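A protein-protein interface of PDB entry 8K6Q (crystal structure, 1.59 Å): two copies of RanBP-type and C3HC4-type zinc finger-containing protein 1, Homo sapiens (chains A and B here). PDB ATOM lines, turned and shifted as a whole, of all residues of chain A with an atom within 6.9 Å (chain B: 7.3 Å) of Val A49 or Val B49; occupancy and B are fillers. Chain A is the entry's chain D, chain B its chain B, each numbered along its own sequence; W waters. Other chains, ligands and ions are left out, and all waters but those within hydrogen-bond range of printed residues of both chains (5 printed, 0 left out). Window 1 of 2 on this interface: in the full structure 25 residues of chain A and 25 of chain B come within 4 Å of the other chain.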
ATOM      1  N   GLU A  15      26.572 -25.948   4.992  1.00  0.00           N
ATOM      2  CA  GLU A  15      26.202 -26.309   3.626  1.00  0.00           C
ATOM      3  C   GLU A  15      25.793 -27.771   3.533  1.00  0.00           C
ATOM      4  O   GLU A  15      24.837 -28.110   2.817  1.00  0.00           O
ATOM      5  CB  GLU A  15      27.360 -25.997   2.686  1.00  0.00           C
ATOM      6  CG  GLU A  15      27.683 -24.512   2.607  1.00  0.00           C
ATOM      7  CD  GLU A  15      26.818 -23.759   1.602  1.00  0.00           C
ATOM      8  OE1 GLU A  15      25.797 -24.310   1.132  1.00  0.00           O
ATOM      9  OE2 GLU A  15      27.168 -22.605   1.267  1.00  0.00           O
ATOM     10  N   MET A  17      24.439 -29.506   5.975  1.00  0.00           N
ATOM     11  CA  MET A  17      23.135 -29.609   6.634  1.00  0.00           C
ATOM     12  C   MET A  17      22.012 -29.070   5.755  1.00  0.00           C
ATOM     13  O   MET A  17      20.898 -29.616   5.759  1.00  0.00           O
ATOM     14  CB  MET A  17      23.180 -28.881   7.978  1.00  0.00           C
ATOM     15  CG  MET A  17      24.096 -29.556   8.988  1.00  0.00           C
ATOM     16  SD  MET A  17      23.340 -31.094   9.564  1.00  0.00           S
ATOM     17  CE  MET A  17      24.215 -32.338   8.635  1.00  0.00           C
ATOM     18  N   ALA A  18      22.272 -27.995   5.005  1.00  0.00           N
ATOM     19  CA  ALA A  18      21.253 -27.468   4.099  1.00  0.00           C
ATOM     20  C   ALA A  18      20.919 -28.471   3.006  1.00  0.00           C
ATOM     21  O   ALA A  18      19.741 -28.684   2.683  1.00  0.00           O
ATOM     22  CB  ALA A  18      21.721 -26.145   3.488  1.00  0.00           C
ATOM     23  N   LEU A  19      21.943 -29.098   2.422  1.00  0.00           N
ATOM     24  CA  LEU A  19      21.702 -30.136   1.422  1.00  0.00           C
ATOM     25  C   LEU A  19      20.998 -31.338   2.032  1.00  0.00           C
ATOM     26  O   LEU A  19      20.077 -31.903   1.423  1.00  0.00           O
ATOM     27  CB  LEU A  19      23.026 -30.575   0.791  1.00  0.00           C
ATOM     28  CG  LEU A  19      23.625 -29.646  -0.250  1.00  0.00           C
ATOM     29  CD1 LEU A  19      25.062 -30.052  -0.532  1.00  0.00           C
ATOM     30  CD2 LEU A  19      22.801 -29.718  -1.530  1.00  0.00           C
ATOM     31  N   LEU A  21      19.031 -31.376   4.672  1.00  0.00           N
ATOM     32  CA  LEU A  21      17.652 -30.990   4.945  1.00  0.00           C
ATOM     33  C   LEU A  21      16.823 -31.014   3.671  1.00  0.00           C
ATOM     34  O   LEU A  21      15.690 -31.511   3.667  1.00  0.00           O
ATOM     35  CB  LEU A  21      17.617 -29.606   5.581  1.00  0.00           C
ATOM     36  CG  LEU A  21      16.224 -29.089   5.967  1.00  0.00           C
ATOM     37  CD1 LEU A  21      15.481 -30.082   6.855  1.00  0.00           C
ATOM     38  CD2 LEU A  21      16.385 -27.763   6.696  1.00  0.00           C
ATOM     39  N   THR A  22      17.385 -30.496   2.574  1.00  0.00           N
ATOM     40  CA  THR A  22      16.684 -30.525   1.291  1.00  0.00           C
ATOM     41  C   THR A  22      16.309 -31.949   0.891  1.00  0.00           C
ATOM     42  O   THR A  22      15.151 -32.227   0.532  1.00  0.00           O
ATOM     43  CB  THR A  22      17.562 -29.889   0.215  1.00  0.00           C
ATOM     44  OG1 THR A  22      17.811 -28.508   0.531  1.00  0.00           O
ATOM     45  CG2 THR A  22      16.883 -29.983  -1.136  1.00  0.00           C
ATOM     46  N   VAL A  25      13.630 -33.537   3.433  1.00  0.00           N
ATOM     47  CA  VAL A  25      12.248 -33.099   3.271  1.00  0.00           C
ATOM     48  C   VAL A  25      11.631 -33.757   2.039  1.00  0.00           C
ATOM     49  O   VAL A  25      10.513 -34.289   2.093  1.00  0.00           O
ATOM     50  CB  VAL A  25      12.169 -31.564   3.205  1.00  0.00           C
ATOM     51  CG1 VAL A  25      10.797 -31.129   2.683  1.00  0.00           C
ATOM     52  CG2 VAL A  25      12.454 -30.975   4.573  1.00  0.00           C
ATOM     53  N   LEU A  40      21.093 -26.170  12.240  1.00  0.00           N
ATOM     54  CA  LEU A  40      21.076 -24.870  11.581  1.00  0.00           C
ATOM     55  C   LEU A  40      20.547 -23.787  12.516  1.00  0.00           C
ATOM     56  O   LEU A  40      21.066 -22.661  12.542  1.00  0.00           O
ATOM     57  CB  LEU A  40      20.224 -24.960  10.306  1.00  0.00           C
ATOM     58  CG  LEU A  40      20.842 -25.828   9.198  1.00  0.00           C
ATOM     59  CD1 LEU A  40      19.803 -26.175   8.140  1.00  0.00           C
ATOM     60  CD2 LEU A  40      22.059 -25.131   8.559  1.00  0.00           C
ATOM     61  N   LEU A  47      19.131 -18.533   6.006  1.00  0.00           N
ATOM     62  CA  LEU A  47      18.778 -19.474   4.961  1.00  0.00           C
ATOM     63  C   LEU A  47      17.931 -18.789   3.902  1.00  0.00           C
ATOM     64  O   LEU A  47      17.232 -17.808   4.172  1.00  0.00           O
ATOM     65  CB  LEU A  47      17.984 -20.670   5.504  1.00  0.00           C
ATOM     66  CG  LEU A  47      18.726 -21.559   6.499  1.00  0.00           C
ATOM     67  CD1 LEU A  47      17.769 -22.637   7.005  1.00  0.00           C
ATOM     68  CD2 LEU A  47      19.976 -22.151   5.845  1.00  0.00           C
ATOM     69  N   SER A  48      18.002 -19.333   2.694  1.00  0.00           N
ATOM     70  CA  SER A  48      17.096 -19.011   1.598  1.00  0.00           C
ATOM     71  C   SER A  48      16.350 -20.296   1.286  1.00  0.00           C
ATOM     72  O   SER A  48      16.949 -21.280   0.838  1.00  0.00           O
ATOM     73  CB  SER A  48      17.873 -18.495   0.382  1.00  0.00           C
ATOM     74  OG  SER A  48      17.039 -18.466  -0.771  1.00  0.00           O
ATOM     75  N   VAL A  49      15.047 -20.321   1.539  1.00  0.00           N
ATOM     76  CA  VAL A  49      14.270 -21.541   1.416  1.00  0.00           C
ATOM     77  C   VAL A  49      13.141 -21.260   0.440  1.00  0.00           C
ATOM     78  O   VAL A  49      12.413 -20.275   0.598  1.00  0.00           O
ATOM     79  CB  VAL A  49      13.725 -22.011   2.780  1.00  0.00           C
ATOM     80  CG1 VAL A  49      12.984 -23.327   2.646  1.00  0.00           C
ATOM     81  CG2 VAL A  49      14.853 -22.158   3.794  1.00  0.00           C
ATOM     82  N   GLN A  50      13.014 -22.098  -0.583  1.00  0.00           N
ATOM     83  CA  GLN A  50      11.902 -21.903  -1.504  1.00  0.00           C
ATOM     84  C   GLN A  50      11.465 -23.232  -2.100  1.00  0.00           C
ATOM     85  O   GLN A  50      12.249 -24.172  -2.210  1.00  0.00           O
ATOM     86  CB  GLN A  50      12.261 -20.936  -2.637  1.00  0.00           C
ATOM     87  CG  GLN A  50      13.299 -21.469  -3.600  1.00  0.00           C
ATOM     88  CD  GLN A  50      13.615 -20.465  -4.704  1.00  0.00           C
ATOM     89  OE1 GLN A  50      13.572 -20.789  -5.889  1.00  0.00           O
ATOM     90  NE2 GLN A  50      13.912 -19.239  -4.314  1.00  0.00           N
ATOM     91  N   LEU A  51      10.193 -23.306  -2.477  1.00  0.00           N
ATOM     92  CA  LEU A  51       9.711 -24.500  -3.152  1.00  0.00           C
ATOM     93  C   LEU A  51      10.258 -24.561  -4.573  1.00  0.00           C
ATOM     94  O   LEU A  51      10.362 -23.540  -5.257  1.00  0.00           O
ATOM     95  CB  LEU A  51       8.186 -24.512  -3.181  1.00  0.00           C
ATOM     96  CG  LEU A  51       7.437 -24.199  -1.886  1.00  0.00           C
ATOM     97  CD1 LEU A  51       5.953 -24.530  -2.045  1.00  0.00           C
ATOM     98  CD2 LEU A  51       8.011 -24.945  -0.712  1.00  0.00           C
ATOM     99  N   LYS A  52      10.631 -25.762  -5.001  1.00  0.00           N
ATOM    100  CA  LYS A  52      11.007 -25.993  -6.392  1.00  0.00           C
ATOM    101  C   LYS A  52       9.780 -25.920  -7.294  1.00  0.00           C
ATOM    102  O   LYS A  52       9.000 -26.871  -7.363  1.00  0.00           O
ATOM    103  CB  LYS A  52      11.683 -27.351  -6.559  1.00  0.00           C
ATOM    104  CG  LYS A  52      12.948 -27.538  -5.746  1.00  0.00           C
ATOM    105  CD  LYS A  52      13.523 -28.930  -5.977  1.00  0.00           C
ATOM    106  CE  LYS A  52      14.536 -29.301  -4.909  1.00  0.00           C
ATOM    107  NZ  LYS A  52      15.721 -28.398  -4.914  1.00  0.00           N
ATOM    108  N   ALA B  14       2.486 -24.579   2.529  1.00  0.00           N
ATOM    109  CA  ALA B  14       3.893 -24.987   2.515  1.00  0.00           C
ATOM    110  C   ALA B  14       4.831 -23.789   2.432  1.00  0.00           C
ATOM    111  O   ALA B  14       5.902 -23.788   3.057  1.00  0.00           O
ATOM    112  CB  ALA B  14       4.160 -25.940   1.354  1.00  0.00           C
ATOM    113  N   GLU B  15       4.463 -22.764   1.660  1.00  0.00           N
ATOM    114  CA  GLU B  15       5.303 -21.569   1.606  1.00  0.00           C
ATOM    115  C   GLU B  15       5.362 -20.860   2.957  1.00  0.00           C
ATOM    116  O   GLU B  15       6.431 -20.381   3.365  1.00  0.00           O
ATOM    117  CB  GLU B  15       4.803 -20.630   0.512  1.00  0.00           C
ATOM    118  CG  GLU B  15       4.995 -21.232  -0.863  1.00  0.00           C
ATOM    119  CD  GLU B  15       4.748 -20.262  -1.999  1.00  0.00           C
ATOM    120  OE1 GLU B  15       4.008 -19.278  -1.800  1.00  0.00           O
ATOM    121  OE2 GLU B  15       5.296 -20.496  -3.101  1.00  0.00           O
ATOM    122  N   MET B  17       5.118 -22.335   5.853  1.00  0.00           N
ATOM    123  CA  MET B  17       5.967 -23.145   6.717  1.00  0.00           C
ATOM    124  C   MET B  17       7.432 -22.982   6.360  1.00  0.00           C
ATOM    125  O   MET B  17       8.294 -23.024   7.248  1.00  0.00           O
ATOM    126  CB  MET B  17       5.562 -24.622   6.646  1.00  0.00           C
ATOM    127  CG  MET B  17       4.184 -24.938   7.206  1.00  0.00           C
ATOM    128  SD  MET B  17       4.036 -24.634   8.977  1.00  0.00           S
ATOM    129  CE  MET B  17       5.335 -25.687   9.572  1.00  0.00           C
ATOM    130  N   ALA B  18       7.746 -22.809   5.070  1.00  0.00           N
ATOM    131  CA  ALA B  18       9.139 -22.560   4.713  1.00  0.00           C
ATOM    132  C   ALA B  18       9.618 -21.230   5.277  1.00  0.00           C
ATOM    133  O   ALA B  18      10.755 -21.124   5.757  1.00  0.00           O
ATOM    134  CB  ALA B  18       9.304 -22.584   3.199  1.00  0.00           C
ATOM    135  N   LEU B  19       8.775 -20.199   5.212  1.00  0.00           N
ATOM    136  CA  LEU B  19       9.135 -18.908   5.790  1.00  0.00           C
ATOM    137  C   LEU B  19       9.271 -19.008   7.306  1.00  0.00           C
ATOM    138  O   LEU B  19      10.171 -18.397   7.896  1.00  0.00           O
ATOM    139  CB  LEU B  19       8.097 -17.847   5.408  1.00  0.00           C
ATOM    140  CG  LEU B  19       8.393 -16.422   5.890  1.00  0.00           C
ATOM    141  CD1 LEU B  19       9.489 -15.765   5.055  1.00  0.00           C
ATOM    142  CD2 LEU B  19       7.130 -15.562   5.893  1.00  0.00           C
ATOM    143  N   LEU B  21      10.168 -21.701   8.971  1.00  0.00           N
ATOM    144  CA  LEU B  21      11.454 -22.362   9.185  1.00  0.00           C
ATOM    145  C   LEU B  21      12.606 -21.371   9.086  1.00  0.00           C
ATOM    146  O   LEU B  21      13.499 -21.359   9.942  1.00  0.00           O
ATOM    147  CB  LEU B  21      11.632 -23.484   8.162  1.00  0.00           C
ATOM    148  CG  LEU B  21      12.995 -24.163   8.144  1.00  0.00           C
ATOM    149  CD1 LEU B  21      13.207 -24.901   9.469  1.00  0.00           C
ATOM    150  CD2 LEU B  21      13.088 -25.128   6.962  1.00  0.00           C
ATOM    151  N   THR B  22      12.617 -20.543   8.032  1.00  0.00           N
ATOM    152  CA  THR B  22      13.703 -19.583   7.851  1.00  0.00           C
ATOM    153  C   THR B  22      13.824 -18.656   9.056  1.00  0.00           C
ATOM    154  O   THR B  22      14.928 -18.416   9.565  1.00  0.00           O
ATOM    155  CB  THR B  22      13.468 -18.766   6.576  1.00  0.00           C
ATOM    156  OG1 THR B  22      13.366 -19.653   5.451  1.00  0.00           O
ATOM    157  CG2 THR B  22      14.617 -17.803   6.353  1.00  0.00           C
ATOM    158  N   VAL B  25      15.033 -20.570  12.246  1.00  0.00           N
ATOM    159  CA  VAL B  25      16.456 -20.861  12.196  1.00  0.00           C
ATOM    160  C   VAL B  25      17.274 -19.598  12.429  1.00  0.00           C
ATOM    161  O   VAL B  25      18.245 -19.605  13.192  1.00  0.00           O
ATOM    162  CB  VAL B  25      16.801 -21.527  10.856  1.00  0.00           C
ATOM    163  CG1 VAL B  25      18.315 -21.585  10.670  1.00  0.00           C
ATOM    164  CG2 VAL B  25      16.220 -22.908  10.819  1.00  0.00           C
ATOM    165  N   LEU B  40       7.263 -30.173   6.990  1.00  0.00           N
ATOM    166  CA  LEU B  40       7.674 -30.160   5.590  1.00  0.00           C
ATOM    167  C   LEU B  40       8.043 -31.554   5.107  1.00  0.00           C
ATOM    168  O   LEU B  40       7.686 -31.949   3.991  1.00  0.00           O
ATOM    169  CB  LEU B  40       8.851 -29.202   5.409  1.00  0.00           C
ATOM    170  CG  LEU B  40       8.415 -27.744   5.577  1.00  0.00           C
ATOM    171  CD1 LEU B  40       9.616 -26.856   5.899  1.00  0.00           C
ATOM    172  CD2 LEU B  40       7.690 -27.268   4.317  1.00  0.00           C
ATOM    173  N   LEU B  47      11.406 -28.922  -1.598  1.00  0.00           N
ATOM    174  CA  LEU B  47      11.966 -27.742  -0.965  1.00  0.00           C
ATOM    175  C   LEU B  47      13.426 -27.594  -1.368  1.00  0.00           C
ATOM    176  O   LEU B  47      14.158 -28.584  -1.444  1.00  0.00           O
ATOM    177  CB  LEU B  47      11.844 -27.873   0.555  1.00  0.00           C
ATOM    178  CG  LEU B  47      11.962 -26.646   1.439  1.00  0.00           C
ATOM    179  CD1 LEU B  47      10.723 -25.808   1.281  1.00  0.00           C
ATOM    180  CD2 LEU B  47      12.162 -27.074   2.889  1.00  0.00           C
ATOM    181  N   SER B  48      13.841 -26.364  -1.654  1.00  0.00           N
ATOM    182  CA  SER B  48      15.250 -26.035  -1.843  1.00  0.00           C
ATOM    183  C   SER B  48      15.726 -25.190  -0.673  1.00  0.00           C
ATOM    184  O   SER B  48      15.289 -24.043  -0.521  1.00  0.00           O
ATOM    185  CB  SER B  48      15.485 -25.275  -3.150  1.00  0.00           C
ATOM    186  OG  SER B  48      16.838 -24.858  -3.217  1.00  0.00           O
ATOM    187  N   VAL B  49      16.663 -25.719   0.125  1.00  0.00           N
ATOM    188  CA  VAL B  49      17.213 -25.002   1.273  1.00  0.00           C
ATOM    189  C   VAL B  49      18.658 -24.646   0.954  1.00  0.00           C
ATOM    190  O   VAL B  49      19.497 -25.537   0.776  1.00  0.00           O
ATOM    191  CB  VAL B  49      17.132 -25.834   2.558  1.00  0.00           C
ATOM    192  CG1 VAL B  49      17.733 -25.047   3.729  1.00  0.00           C
ATOM    193  CG2 VAL B  49      15.701 -26.201   2.857  1.00  0.00           C
ATOM    194  N   GLN B  50      18.955 -23.353   0.848  1.00  0.00           N
ATOM    195  CA  GLN B  50      20.322 -22.899   0.606  1.00  0.00           C
ATOM    196  C   GLN B  50      20.734 -21.866   1.647  1.00  0.00           C
ATOM    197  O   GLN B  50      19.908 -21.302   2.367  1.00  0.00           O
ATOM    198  CB  GLN B  50      20.466 -22.300  -0.787  1.00  0.00           C
ATOM    199  CG  GLN B  50      20.148 -23.293  -1.875  1.00  0.00           C
ATOM    200  CD  GLN B  50      20.434 -22.729  -3.247  1.00  0.00           C
ATOM    201  OE1 GLN B  50      20.731 -21.542  -3.392  1.00  0.00           O
ATOM    202  NE2 GLN B  50      20.346 -23.575  -4.264  1.00  0.00           N
ATOM    203  N   LEU B  51      22.036 -21.628   1.745  1.00  0.00           N
ATOM    204  CA  LEU B  51      22.476 -20.543   2.596  1.00  0.00           C
ATOM    205  C   LEU B  51      22.111 -19.220   1.936  1.00  0.00           C
ATOM    206  O   LEU B  51      22.226 -19.064   0.713  1.00  0.00           O
ATOM    207  CB  LEU B  51      23.978 -20.643   2.862  1.00  0.00           C
ATOM    208  CG  LEU B  51      24.338 -21.365   4.159  1.00  0.00           C
ATOM    209  CD1 LEU B  51      23.764 -22.772   4.258  1.00  0.00           C
ATOM    210  CD2 LEU B  51      25.855 -21.392   4.314  1.00  0.00           C
ATOM    211  N   LYS B  52      21.627 -18.280   2.746  1.00  0.00           N
ATOM    212  CA  LYS B  52      21.248 -16.960   2.234  1.00  0.00           C
ATOM    213  C   LYS B  52      22.473 -16.203   1.738  1.00  0.00           C
ATOM    214  O   LYS B  52      23.502 -16.173   2.424  1.00  0.00           O
ATOM    215  CB  LYS B  52      20.539 -16.148   3.322  1.00  0.00           C
ATOM    216  CG  LYS B  52      19.868 -14.866   2.820  1.00  0.00           C
ATOM    217  CD  LYS B  52      19.174 -14.129   3.956  1.00  0.00           C
ATOM    218  CE  LYS B  52      18.310 -12.985   3.437  1.00  0.00           C
ATOM    219  NZ  LYS B  52      17.382 -12.481   4.488  1.00  0.00           N
HETATM  220  O   HOH W   1       8.594 -20.740  -2.637  1.00  0.00           O
HETATM  221  O   HOH W   2      10.614 -18.962   2.867  1.00  0.00           O
HETATM  222  O   HOH W   3      23.780 -23.105   0.091  1.00  0.00           O
HETATM  223  O   HOH W   4      13.206 -30.908  -1.035  1.00  0.00           O
HETATM  224  O   HOH W   5      17.444 -18.563   8.323  1.00  0.00           O
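Among the printed residues, merely in contact across the chains: Thr A22 with Leu B47, Val A49 with Ser B48, Val A49 with Thr B22, Leu A47 with Gln B50, Leu A47 with Thr B22, Val A25 with Leu B40, Leu A51 with Leu B47, Leu A40 with Val B25, Glu A15 with Leu B51, Lys A52 with Leu B47, Ala A18 with Val B49, Lys A52 with Ser B48, Val A49 with Leu B47, Leu A51 with Glu B15, Gln A50 with Leu B47, Ser A48 with Val B49, Leu A47 with Lys B52, Ser A48 with Lys B52, Val A49 with Ala B18, Leu A47 with Val B25 and Val A49 with Val B49.
Printed residues of chain B that touch a printed residue of chain A: Glu B15, Ala B18, Thr B22, Val B25, Leu B40, Leu B47, Ser B48, Val B49, Gln B50, Leu B51 and Lys B52.
Hydrophobic or aromatic side chains of chain A that line the printed part of chain B: Ala A18, Val A25, Leu A40, Leu A47, Val A49 and Leu A51.
Among the printed residues, 25 pairs touch across the chains.
Among the printed residues, no Asp or Glu carboxylate lies within 4 Å of a Lys or Arg side-chain nitrogen of the other chain.
The side-chain hydroxyl (OG1) of Thr A22 lies within hydrogen-bond range of the backbone carbonyl oxygen (O) of Ala A18 (2.9 Å).
O of Ala B18 lies within hydrogen-bond range of OG1 of Thr B22 (3.0 Å).
Val A49 touches five residues of chain B.
Of chain A, only Ala A18, Thr A22, Ser A48 and Val A49 come within 4 Å of Val B49.
Of the printed residues of chain A, Val B25 touches Leu A40 and Leu A47.
Printed residues of chain A within 4 Å of Ser B48: Ser A48 (3.5 Å), Val A49 (3.3 Å), Gln A50 (2.8 Å) and Lys A52 (3.6 Å).
Of the printed residues of chain A, Leu B47 touches Thr A22, Val A49, Gln A50, Leu A51 and Lys A52.
Of the printed residues of chain A, Thr B22 touches Leu A47 and Val A49.
Of the printed residues of chain B, Thr A22 touches Leu B47 (3.1 Å) and Val B49 (3.0 Å).
Leu B21 touches none of the printed residues of chain A.
Leu A21 touches none of the printed residues of chain B.
The nearest residue of chain B that does not touch Val A49 is Leu B21 (4.7 Å).
N of Val B49 sits at hydrogen-bond distance from OG1 of Thr A22 (3.0 Å).
The backbone carbonyl oxygen (O) of Gln B50 sits at hydrogen-bond distance from the backbone NH (N) of Ser A48.
The backbone carbonyl oxygen (O) of Ser A48 sits close to the backbone carbonyl oxygen (O) of Ser B48, 3.5 Å away.
The backbone NH (N) of Ser B48 sits at hydrogen-bond distance from the backbone carbonyl oxygen (O) of Gln A50 (2.8 Å).
Water W4 bridges O of Leu B47 (2.5 Å) and O of Thr A22 (2.8 Å).
Water W3 bridges OE1 of Glu A15 (2.6 Å) and N of Leu B51 (2.8 Å).
Water W5 lies within hydrogen-bond range of O of Thr B22 (2.8 Å) and N of Leu A47 (2.9 Å).
Water W1 lies within hydrogen-bond range of the backbone NH (N) of Leu A51 (3.0 Å) and the side-chain carboxylate (OE2) of Glu B15 (3.3 Å).
Water W2 bridges the backbone carbonyl oxygen of Val A49 (3.2 Å) and the backbone NH of Leu B19 (3.2 Å).
Leu A47 touches Val B25, but with the chains exchanged Val A25 does not touch Leu B47 (4.03 Å).
Leu A47 touches Gln B50, and with the chains exchanged Gln A50 touches Leu B47.
Ser B48 touches its own counterpart, Ser A48.
Val A49 touches Leu B47, but with the chains exchanged Leu A47 does not touch Val B49 (4.1 Å).
Positions printed for both chains: 15, 17, 18, 19, 21, 22, 25, 40, 47, 48, 49, 50, 51 and 52.
Of the 25 pairs that touch across the chains among the printed residues, 22 have their exchanged pair printed and touching as well.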
